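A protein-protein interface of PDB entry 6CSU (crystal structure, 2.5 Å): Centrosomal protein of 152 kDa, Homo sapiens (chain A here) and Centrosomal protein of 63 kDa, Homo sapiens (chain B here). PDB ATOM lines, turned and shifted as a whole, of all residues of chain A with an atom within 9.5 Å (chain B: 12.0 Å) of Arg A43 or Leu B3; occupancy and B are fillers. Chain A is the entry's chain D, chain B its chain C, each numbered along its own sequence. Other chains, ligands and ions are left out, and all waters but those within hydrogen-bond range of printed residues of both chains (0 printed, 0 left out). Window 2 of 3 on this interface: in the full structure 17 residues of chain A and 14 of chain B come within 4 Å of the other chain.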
ATOM      1  N   ARG A  32      13.784  11.754 -19.230  1.00  0.00           N
ATOM      2  CA  ARG A  32      12.906  12.003 -18.093  1.00  0.00           C
ATOM      3  C   ARG A  32      11.693  12.824 -18.509  1.00  0.00           C
ATOM      4  O   ARG A  32      10.590  12.619 -17.991  1.00  0.00           O
ATOM      5  CB  ARG A  32      13.684  12.695 -16.971  1.00  0.00           C
ATOM      6  CG  ARG A  32      14.824  11.844 -16.423  1.00  0.00           C
ATOM      7  CD  ARG A  32      15.624  12.516 -15.308  1.00  0.00           C
ATOM      8  NE  ARG A  32      15.304  13.928 -15.120  1.00  0.00           N
ATOM      9  CZ  ARG A  32      14.452  14.377 -14.207  1.00  0.00           C
ATOM     10  NH1 ARG A  32      13.822  13.522 -13.415  1.00  0.00           N
ATOM     11  NH2 ARG A  32      14.216  15.673 -14.096  1.00  0.00           N
ATOM     12  N   ALA A  33      11.874  13.753 -19.453  1.00  0.00           N
ATOM     13  CA  ALA A  33      10.734  14.497 -19.980  1.00  0.00           C
ATOM     14  C   ALA A  33       9.823  13.592 -20.798  1.00  0.00           C
ATOM     15  O   ALA A  33       8.593  13.695 -20.710  1.00  0.00           O
ATOM     16  CB  ALA A  33      11.213  15.674 -20.827  1.00  0.00           C
ATOM     17  N   GLU A  35       9.517  10.358 -20.390  1.00  0.00           N
ATOM     18  CA  GLU A  35       8.827   9.521 -19.416  1.00  0.00           C
ATOM     19  C   GLU A  35       7.631  10.242 -18.815  1.00  0.00           C
ATOM     20  O   GLU A  35       6.615   9.608 -18.510  1.00  0.00           O
ATOM     21  CB  GLU A  35       9.789   9.075 -18.315  1.00  0.00           C
ATOM     22  CG  GLU A  35      10.193   7.610 -18.404  1.00  0.00           C
ATOM     23  CD  GLU A  35       8.998   6.675 -18.393  1.00  0.00           C
ATOM     24  OE1 GLU A  35       8.000   6.985 -17.706  1.00  0.00           O
ATOM     25  OE2 GLU A  35       9.052   5.632 -19.078  1.00  0.00           O
ATOM     26  N   MET A  36       7.723  11.564 -18.651  1.00  0.00           N
ATOM     27  CA  MET A  36       6.595  12.328 -18.133  1.00  0.00           C
ATOM     28  C   MET A  36       5.460  12.421 -19.140  1.00  0.00           C
ATOM     29  O   MET A  36       4.319  12.684 -18.748  1.00  0.00           O
ATOM     30  CB  MET A  36       7.050  13.732 -17.724  1.00  0.00           C
ATOM     31  CG  MET A  36       6.242  14.343 -16.597  1.00  0.00           C
ATOM     32  SD  MET A  36       7.088  14.215 -15.011  1.00  0.00           S
ATOM     33  CE  MET A  36       7.082  12.447 -14.708  1.00  0.00           C
ATOM     34  N   VAL A  37       5.749  12.218 -20.424  1.00  0.00           N
ATOM     35  CA  VAL A  37       4.692  12.194 -21.427  1.00  0.00           C
ATOM     36  C   VAL A  37       3.907  10.892 -21.335  1.00  0.00           C
ATOM     37  O   VAL A  37       2.670  10.893 -21.347  1.00  0.00           O
ATOM     38  CB  VAL A  37       5.286  12.398 -22.830  1.00  0.00           C
ATOM     39  CG1 VAL A  37       4.183  12.382 -23.871  1.00  0.00           C
ATOM     40  CG2 VAL A  37       6.077  13.699 -22.882  1.00  0.00           C
ATOM     41  N   LYS A  38       4.613   9.764 -21.241  1.00  0.00           N
ATOM     42  CA  LYS A  38       3.952   8.472 -21.088  1.00  0.00           C
ATOM     43  C   LYS A  38       3.098   8.434 -19.829  1.00  0.00           C
ATOM     44  O   LYS A  38       1.906   8.107 -19.878  1.00  0.00           O
ATOM     45  CB  LYS A  38       4.985   7.344 -21.050  1.00  0.00           C
ATOM     46  CG  LYS A  38       5.429   6.867 -22.411  1.00  0.00           C
ATOM     47  CD  LYS A  38       6.315   5.630 -22.313  1.00  0.00           C
ATOM     48  CE  LYS A  38       5.545   4.381 -21.880  1.00  0.00           C
ATOM     49  NZ  LYS A  38       6.394   3.148 -21.978  1.00  0.00           N
ATOM     50  N   ALA A  39       3.705   8.772 -18.685  1.00  0.00           N
ATOM     51  CA  ALA A  39       3.027   8.645 -17.398  1.00  0.00           C
ATOM     52  C   ALA A  39       1.689   9.366 -17.372  1.00  0.00           C
ATOM     53  O   ALA A  39       0.795   8.986 -16.606  1.00  0.00           O
ATOM     54  CB  ALA A  39       3.918   9.182 -16.277  1.00  0.00           C
ATOM     55  N   GLU A  40       1.527  10.401 -18.195  1.00  0.00           N
ATOM     56  CA  GLU A  40       0.314  11.204 -18.179  1.00  0.00           C
ATOM     57  C   GLU A  40      -0.723  10.748 -19.196  1.00  0.00           C
ATOM     58  O   GLU A  40      -1.924  10.848 -18.926  1.00  0.00           O
ATOM     59  CB  GLU A  40       0.644  12.677 -18.416  1.00  0.00           C
ATOM     60  CG  GLU A  40      -0.438  13.609 -17.884  1.00  0.00           C
ATOM     61  CD  GLU A  40      -0.525  14.905 -18.659  1.00  0.00           C
ATOM     62  OE1 GLU A  40       0.457  15.233 -19.358  1.00  0.00           O
ATOM     63  OE2 GLU A  40      -1.582  15.573 -18.601  1.00  0.00           O
ATOM     64  N   VAL A  41      -0.299  10.259 -20.365  1.00  0.00           N
ATOM     65  CA  VAL A  41      -1.235   9.563 -21.245  1.00  0.00           C
ATOM     66  C   VAL A  41      -1.896   8.423 -20.486  1.00  0.00           C
ATOM     67  O   VAL A  41      -3.083   8.125 -20.675  1.00  0.00           O
ATOM     68  CB  VAL A  41      -0.515   9.065 -22.514  1.00  0.00           C
ATOM     69  CG1 VAL A  41      -1.311   7.958 -23.181  1.00  0.00           C
ATOM     70  CG2 VAL A  41      -0.315  10.210 -23.481  1.00  0.00           C
ATOM     71  N   LEU A  42      -1.140   7.790 -19.586  1.00  0.00           N
ATOM     72  CA  LEU A  42      -1.695   6.756 -18.724  1.00  0.00           C
ATOM     73  C   LEU A  42      -2.671   7.323 -17.702  1.00  0.00           C
ATOM     74  O   LEU A  42      -3.570   6.607 -17.246  1.00  0.00           O
ATOM     75  CB  LEU A  42      -0.567   6.011 -18.019  1.00  0.00           C
ATOM     76  CG  LEU A  42      -0.146   4.706 -18.690  1.00  0.00           C
ATOM     77  CD1 LEU A  42       0.155   4.914 -20.165  1.00  0.00           C
ATOM     78  CD2 LEU A  42       1.055   4.128 -17.973  1.00  0.00           C
ATOM     79  N   ARG A  43      -2.514   8.594 -17.323  1.00  0.00           N
ATOM     80  CA  ARG A  43      -3.472   9.210 -16.412  1.00  0.00           C
ATOM     81  C   ARG A  43      -4.790   9.570 -17.089  1.00  0.00           C
ATOM     82  O   ARG A  43      -5.772   9.835 -16.383  1.00  0.00           O
ATOM     83  CB  ARG A  43      -2.864  10.451 -15.751  1.00  0.00           C
ATOM     84  CG  ARG A  43      -1.867  10.127 -14.639  1.00  0.00           C
ATOM     85  CD  ARG A  43      -1.774  11.240 -13.596  1.00  0.00           C
ATOM     86  NE  ARG A  43      -1.503  12.544 -14.195  1.00  0.00           N
ATOM     87  CZ  ARG A  43      -2.424  13.485 -14.383  1.00  0.00           C
ATOM     88  NH1 ARG A  43      -3.678  13.271 -14.011  1.00  0.00           N
ATOM     89  NH2 ARG A  43      -2.088  14.640 -14.940  1.00  0.00           N
ATOM     90  N   GLU A  44      -4.841   9.587 -18.427  1.00  0.00           N
ATOM     91  CA  GLU A  44      -6.114   9.710 -19.127  1.00  0.00           C
ATOM     92  C   GLU A  44      -6.939   8.443 -19.058  1.00  0.00           C
ATOM     93  O   GLU A  44      -8.144   8.495 -19.322  1.00  0.00           O
ATOM     94  CB  GLU A  44      -5.926  10.025 -20.603  1.00  0.00           C
ATOM     95  CG  GLU A  44      -4.860  11.009 -20.935  1.00  0.00           C
ATOM     96  CD  GLU A  44      -4.680  11.079 -22.425  1.00  0.00           C
ATOM     97  OE1 GLU A  44      -5.709  11.093 -23.132  1.00  0.00           O
ATOM     98  OE2 GLU A  44      -3.523  11.099 -22.889  1.00  0.00           O
ATOM     99  N   ARG A  45      -6.308   7.301 -18.785  1.00  0.00           N
ATOM    100  CA  ARG A  45      -7.070   6.087 -18.533  1.00  0.00           C
ATOM    101  C   ARG A  45      -8.120   6.344 -17.465  1.00  0.00           C
ATOM    102  O   ARG A  45      -9.274   5.923 -17.591  1.00  0.00           O
ATOM    103  CB  ARG A  45      -6.135   4.954 -18.115  1.00  0.00           C
ATOM    104  CG  ARG A  45      -5.427   4.268 -19.264  1.00  0.00           C
ATOM    105  CD  ARG A  45      -4.209   3.538 -18.747  1.00  0.00           C
ATOM    106  NE  ARG A  45      -3.834   2.405 -19.581  1.00  0.00           N
ATOM    107  CZ  ARG A  45      -3.136   1.367 -19.135  1.00  0.00           C
ATOM    108  NH1 ARG A  45      -2.756   1.329 -17.866  1.00  0.00           N
ATOM    109  NH2 ARG A  45      -2.825   0.368 -19.948  1.00  0.00           N
ATOM    110  N   GLN A  46      -7.733   7.069 -16.413  1.00  0.00           N
ATOM    111  CA  GLN A  46      -8.690   7.469 -15.389  1.00  0.00           C
ATOM    112  C   GLN A  46      -9.806   8.325 -15.978  1.00  0.00           C
ATOM    113  O   GLN A  46     -10.971   8.192 -15.588  1.00  0.00           O
ATOM    114  CB  GLN A  46      -7.963   8.213 -14.268  1.00  0.00           C
ATOM    115  CG  GLN A  46      -7.091   7.309 -13.404  1.00  0.00           C
ATOM    116  CD  GLN A  46      -5.990   8.061 -12.675  1.00  0.00           C
ATOM    117  OE1 GLN A  46      -5.904   9.289 -12.743  1.00  0.00           O
ATOM    118  NE2 GLN A  46      -5.134   7.320 -11.978  1.00  0.00           N
ATOM    119  N   GLU A  47      -9.473   9.198 -16.932  1.00  0.00           N
ATOM    120  CA  GLU A  47     -10.491  10.032 -17.565  1.00  0.00           C
ATOM    121  C   GLU A  47     -11.369   9.211 -18.501  1.00  0.00           C
ATOM    122  O   GLU A  47     -12.603   9.298 -18.446  1.00  0.00           O
ATOM    123  CB  GLU A  47      -9.833  11.186 -18.322  1.00  0.00           C
ATOM    124  CG  GLU A  47     -10.775  11.957 -19.242  1.00  0.00           C
ATOM    125  CD  GLU A  47     -11.369  13.187 -18.584  1.00  0.00           C
ATOM    126  OE1 GLU A  47     -11.124  13.399 -17.377  1.00  0.00           O
ATOM    127  OE2 GLU A  47     -12.075  13.951 -19.277  1.00  0.00           O
ATOM    128  N   THR A  48     -10.750   8.407 -19.372  1.00  0.00           N
ATOM    129  CA  THR A  48     -11.525   7.570 -20.283  1.00  0.00           C
ATOM    130  C   THR A  48     -12.367   6.551 -19.527  1.00  0.00           C
ATOM    131  O   THR A  48     -13.453   6.181 -19.988  1.00  0.00           O
ATOM    132  CB  THR A  48     -10.601   6.859 -21.275  1.00  0.00           C
ATOM    133  OG1 THR A  48      -9.689   6.015 -20.562  1.00  0.00           O
ATOM    134  CG2 THR A  48      -9.820   7.870 -22.104  1.00  0.00           C
ATOM    135  N   ALA A  49     -11.883   6.083 -18.374  1.00  0.00           N
ATOM    136  CA  ALA A  49     -12.698   5.214 -17.531  1.00  0.00           C
ATOM    137  C   ALA A  49     -13.918   5.960 -17.011  1.00  0.00           C
ATOM    138  O   ALA A  49     -15.038   5.437 -17.030  1.00  0.00           O
ATOM    139  CB  ALA A  49     -11.866   4.664 -16.373  1.00  0.00           C
ATOM    140  N   ARG A  50     -13.715   7.195 -16.543  1.00  0.00           N
ATOM    141  CA  ARG A  50     -14.835   8.020 -16.108  1.00  0.00           C
ATOM    142  C   ARG A  50     -15.837   8.239 -17.233  1.00  0.00           C
ATOM    143  O   ARG A  50     -17.039   8.371 -16.981  1.00  0.00           O
ATOM    144  CB  ARG A  50     -14.321   9.364 -15.587  1.00  0.00           C
ATOM    145  CG  ARG A  50     -15.262  10.056 -14.623  1.00  0.00           C
ATOM    146  CD  ARG A  50     -15.350   9.292 -13.317  1.00  0.00           C
ATOM    147  NE  ARG A  50     -16.360   9.852 -12.427  1.00  0.00           N
ATOM    148  CZ  ARG A  50     -17.645   9.514 -12.455  1.00  0.00           C
ATOM    149  NH1 ARG A  50     -18.077   8.615 -13.332  1.00  0.00           N
ATOM    150  NH2 ARG A  50     -18.498  10.076 -11.610  1.00  0.00           N
ATOM    151  N   ALA B   1       0.238  18.072 -10.150  1.00  0.00           N
ATOM    152  CA  ALA B   1       0.208  17.172  -9.003  1.00  0.00           C
ATOM    153  C   ALA B   1       1.577  16.543  -8.788  1.00  0.00           C
ATOM    154  O   ALA B   1       2.606  17.205  -8.949  1.00  0.00           O
ATOM    155  CB  ALA B   1      -0.872  16.090  -9.180  1.00  0.00           C
ATOM    156  N   CYS B   2       1.591  15.258  -8.437  1.00  0.00           N
ATOM    157  CA  CYS B   2       2.756  14.670  -7.790  1.00  0.00           C
ATOM    158  C   CYS B   2       3.752  14.058  -8.766  1.00  0.00           C
ATOM    159  O   CYS B   2       4.879  13.761  -8.366  1.00  0.00           O
ATOM    160  CB  CYS B   2       2.292  13.624  -6.776  1.00  0.00           C
ATOM    161  SG  CYS B   2       1.065  14.300  -5.588  1.00  0.00           S
ATOM    162  N   LEU B   3       3.376  13.876 -10.036  1.00  0.00           N
ATOM    163  CA  LEU B   3       4.366  13.555 -11.063  1.00  0.00           C
ATOM    164  C   LEU B   3       5.352  14.696 -11.235  1.00  0.00           C
ATOM    165  O   LEU B   3       6.565  14.478 -11.281  1.00  0.00           O
ATOM    166  CB  LEU B   3       3.690  13.257 -12.409  1.00  0.00           C
ATOM    167  CG  LEU B   3       2.982  11.933 -12.747  1.00  0.00           C
ATOM    168  CD1 LEU B   3       2.128  12.119 -14.006  1.00  0.00           C
ATOM    169  CD2 LEU B   3       3.924  10.718 -12.902  1.00  0.00           C
ATOM    170  N   ASN B   4       4.850  15.934 -11.295  1.00  0.00           N
ATOM    171  CA  ASN B   4       5.683  17.063 -11.697  1.00  0.00           C
ATOM    172  C   ASN B   4       6.530  17.562 -10.536  1.00  0.00           C
ATOM    173  O   ASN B   4       7.684  17.967 -10.735  1.00  0.00           O
ATOM    174  CB  ASN B   4       4.808  18.203 -12.225  1.00  0.00           C
ATOM    175  CG  ASN B   4       3.820  17.754 -13.277  1.00  0.00           C
ATOM    176  OD1 ASN B   4       2.738  17.249 -12.956  1.00  0.00           O
ATOM    177  ND2 ASN B   4       4.171  17.951 -14.544  1.00  0.00           N
ATOM    178  N   THR B   5       5.971  17.584  -9.325  1.00  0.00           N
ATOM    179  CA  THR B   5       6.765  17.949  -8.159  1.00  0.00           C
ATOM    180  C   THR B   5       7.903  16.960  -7.960  1.00  0.00           C
ATOM    181  O   THR B   5       9.046  17.359  -7.723  1.00  0.00           O
ATOM    182  CB  THR B   5       5.879  18.015  -6.915  1.00  0.00           C
ATOM    183  OG1 THR B   5       5.351  16.714  -6.621  1.00  0.00           O
ATOM    184  CG2 THR B   5       4.731  18.952  -7.154  1.00  0.00           C
ATOM    185  N   ARG B   6       7.614  15.664  -8.065  1.00  0.00           N
ATOM    186  CA  ARG B   6       8.664  14.657  -7.965  1.00  0.00           C
ATOM    187  C   ARG B   6       9.644  14.768  -9.125  1.00  0.00           C
ATOM    188  O   ARG B   6      10.827  14.460  -8.964  1.00  0.00           O
ATOM    189  CB  ARG B   6       8.058  13.251  -7.924  1.00  0.00           C
ATOM    190  CG  ARG B   6       9.046  12.159  -7.553  1.00  0.00           C
ATOM    191  CD  ARG B   6       9.079  11.042  -8.595  1.00  0.00           C
ATOM    192  NE  ARG B   6       7.979  10.091  -8.438  1.00  0.00           N
ATOM    193  CZ  ARG B   6       7.620   9.204  -9.362  1.00  0.00           C
ATOM    194  NH1 ARG B   6       8.266   9.144 -10.517  1.00  0.00           N
ATOM    195  NH2 ARG B   6       6.609   8.377  -9.134  1.00  0.00           N
ATOM    196  N   PHE B   7       9.171  15.205 -10.295  1.00  0.00           N
ATOM    197  CA  PHE B   7      10.075  15.502 -11.403  1.00  0.00           C
ATOM    198  C   PHE B   7      11.030  16.615 -11.018  1.00  0.00           C
ATOM    199  O   PHE B   7      12.238  16.515 -11.245  1.00  0.00           O
ATOM    200  CB  PHE B   7       9.266  15.889 -12.646  1.00  0.00           C
ATOM    201  CG  PHE B   7      10.096  16.269 -13.847  1.00  0.00           C
ATOM    202  CD1 PHE B   7      10.538  15.298 -14.732  1.00  0.00           C
ATOM    203  CD2 PHE B   7      10.417  17.598 -14.105  1.00  0.00           C
ATOM    204  CE1 PHE B   7      11.294  15.641 -15.845  1.00  0.00           C
ATOM    205  CE2 PHE B   7      11.174  17.945 -15.221  1.00  0.00           C
ATOM    206  CZ  PHE B   7      11.609  16.965 -16.089  1.00  0.00           C
ATOM    207  N   LEU B   8      10.498  17.675 -10.407  1.00  0.00           N
ATOM    208  CA  LEU B   8      11.319  18.818 -10.029  1.00  0.00           C
ATOM    209  C   LEU B   8      12.348  18.427  -8.979  1.00  0.00           C
ATOM    210  O   LEU B   8      13.524  18.792  -9.081  1.00  0.00           O
ATOM    211  CB  LEU B   8      10.425  19.945  -9.512  1.00  0.00           C
ATOM    212  CG  LEU B   8      11.110  21.261  -9.152  1.00  0.00           C
ATOM    213  CD1 LEU B   8      11.531  22.003 -10.402  1.00  0.00           C
ATOM    214  CD2 LEU B   8      10.205  22.132  -8.305  1.00  0.00           C
ATOM    215  N   GLU B   9      11.913  17.692  -7.951  1.00  0.00           N
ATOM    216  CA  GLU B   9      12.831  17.226  -6.917  1.00  0.00           C
ATOM    217  C   GLU B   9      13.980  16.434  -7.519  1.00  0.00           C
ATOM    218  O   GLU B   9      15.128  16.550  -7.076  1.00  0.00           O
ATOM    219  CB  GLU B   9      12.074  16.379  -5.896  1.00  0.00           C
ATOM    220  CG  GLU B   9      10.987  17.135  -5.162  1.00  0.00           C
ATOM    221  CD  GLU B   9      10.110  16.222  -4.328  1.00  0.00           C
ATOM    222  OE1 GLU B   9      10.290  14.989  -4.415  1.00  0.00           O
ATOM    223  OE2 GLU B   9       9.240  16.734  -3.593  1.00  0.00           O
ATOM    224  N   GLU B  10      13.686  15.626  -8.540  1.00  0.00           N
ATOM    225  CA  GLU B  10      14.738  14.915  -9.254  1.00  0.00           C
ATOM    226  C   GLU B  10      15.658  15.889  -9.980  1.00  0.00           C
ATOM    227  O   GLU B  10      16.884  15.765  -9.910  1.00  0.00           O
ATOM    228  CB  GLU B  10      14.122  13.920 -10.236  1.00  0.00           C
ATOM    229  CG  GLU B  10      13.385  12.765  -9.585  1.00  0.00           C
ATOM    230  CD  GLU B  10      12.500  12.016 -10.566  1.00  0.00           C
ATOM    231  OE1 GLU B  10      12.394  12.461 -11.728  1.00  0.00           O
ATOM    232  OE2 GLU B  10      11.918  10.983 -10.172  1.00  0.00           O
ATOM    233  N   GLU B  11      15.075  16.861 -10.691  1.00  0.00           N
ATOM    234  CA  GLU B  11      15.873  17.887 -11.359  1.00  0.00           C
ATOM    235  C   GLU B  11      16.850  18.533 -10.388  1.00  0.00           C
ATOM    236  O   GLU B  11      18.030  18.720 -10.702  1.00  0.00           O
ATOM    237  CB  GLU B  11      14.958  18.954 -11.969  1.00  0.00           C
ATOM    238  CG  GLU B  11      14.456  18.667 -13.375  1.00  0.00           C
ATOM    239  CD  GLU B  11      15.523  18.840 -14.437  1.00  0.00           C
ATOM    240  OE1 GLU B  11      16.504  19.572 -14.183  1.00  0.00           O
ATOM    241  OE2 GLU B  11      15.381  18.242 -15.526  1.00  0.00           O
ATOM    242  N   GLU B  12      16.362  18.874  -9.191  1.00  0.00           N
ATOM    243  CA  GLU B  12      17.200  19.503  -8.176  1.00  0.00           C
ATOM    244  C   GLU B  12      18.400  18.632  -7.834  1.00  0.00           C
ATOM    245  O   GLU B  12      19.519  19.135  -7.677  1.00  0.00           O
ATOM    246  CB  GLU B  12      16.373  19.771  -6.921  1.00  0.00           C
ATOM    247  CG  GLU B  12      16.739  21.041  -6.187  1.00  0.00           C
ATOM    248  CD  GLU B  12      15.931  22.223  -6.667  1.00  0.00           C
ATOM    249  OE1 GLU B  12      14.706  22.069  -6.858  1.00  0.00           O
ATOM    250  OE2 GLU B  12      16.520  23.305  -6.864  1.00  0.00           O
ATOM    251  N   ARG B  14      19.804  16.180  -9.706  1.00  0.00           N
ATOM    252  CA  ARG B  14      20.694  16.124 -10.856  1.00  0.00           C
ATOM    253  C   ARG B  14      21.417  17.442 -11.075  1.00  0.00           C
ATOM    254  O   ARG B  14      22.537  17.439 -11.592  1.00  0.00           O
ATOM    255  CB  ARG B  14      19.906  15.742 -12.110  1.00  0.00           C
ATOM    256  CG  ARG B  14      19.070  14.484 -11.946  1.00  0.00           C
ATOM    257  CD  ARG B  14      18.414  14.048 -13.244  1.00  0.00           C
ATOM    258  NE  ARG B  14      17.997  15.176 -14.067  1.00  0.00           N
ATOM    259  CZ  ARG B  14      18.525  15.456 -15.252  1.00  0.00           C
ATOM    260  NH1 ARG B  14      19.481  14.681 -15.746  1.00  0.00           N
ATOM    261  NH2 ARG B  14      18.095  16.501 -15.945  1.00  0.00           N
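The side-chain carboxylate (OE1) of Glu B10 lies within salt-bridge range of the guanidinium group (NH1) of Arg A32, at 2.5 Å. NH2 of Arg A32 lies within salt-bridge range of OE2 of Glu B11, at 3.2 Å. The guanidinium group of Arg B14 sits close to the guanidinium group of Arg A32 (3.1 Å). The side-chain sulfur (SD) of Met A36 lies close to the backbone carbonyl oxygen (O) of Leu B3 (3.8 Å).
Printed residues of chain B within 4 Å of Arg A43: Leu B3 (3.7 Å). Of chain B, only Leu B3 (3.8 Å) and Phe B7 (3.6 Å) come within 4 Å of Met A36. No residue of chain B comes within 4 Å of Glu A40. No residue of chain B comes within 4 Å of Val A41. No residue of chain B comes within 4 Å of Leu A42. No residue of chain B comes within 4 Å of Glu A44. No residue of chain B comes within 4 Å of Gln A46. No residue of chain A comes within 4 Å of Cys B2. Of the printed residues of chain B, Arg A32 touches Phe B7 (3.4 Å), Glu B10 (2.5 Å), Glu B11 (3.1 Å) and Arg B14 (3.1 Å). Of the printed residues of chain A, Glu B11 touches Arg A32 (3.1 Å). Printed residues of chain A within 4 Å of Arg B14: Arg A32. Printed residues of chain A within 4 Å of Glu B10: Arg A32 (2.5 Å). Of the printed residues of chain A, Phe B7 touches Arg A32 (3.4 Å) and Met A36 (3.6 Å). Glu B9 touches none of the printed residues of chain A.
Among the printed residues, pairs that only touch across the chains: Arg A32 with Phe B7, Met A36 with Phe B7, Arg A43 with Leu B3 and Ala A39 with Leu B3.
Hydrophobic or aromatic side chains of chain A that line the printed part of chain B: Met A36 and Ala A39. Hydrophobic or aromatic side chains of chain B that line the printed part of chain A: Leu B3 and Phe B7.
The guanidinium group (NH2) of Arg A43 lies within salt-bridge range of the side-chain carboxylate (OE2) of Glu A40, at 3.8 Å. The guanidinium group (NH2) of Arg B14 is in salt-bridge range of the side-chain carboxylate (OE2) of Glu B11, 3.3 Å away.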
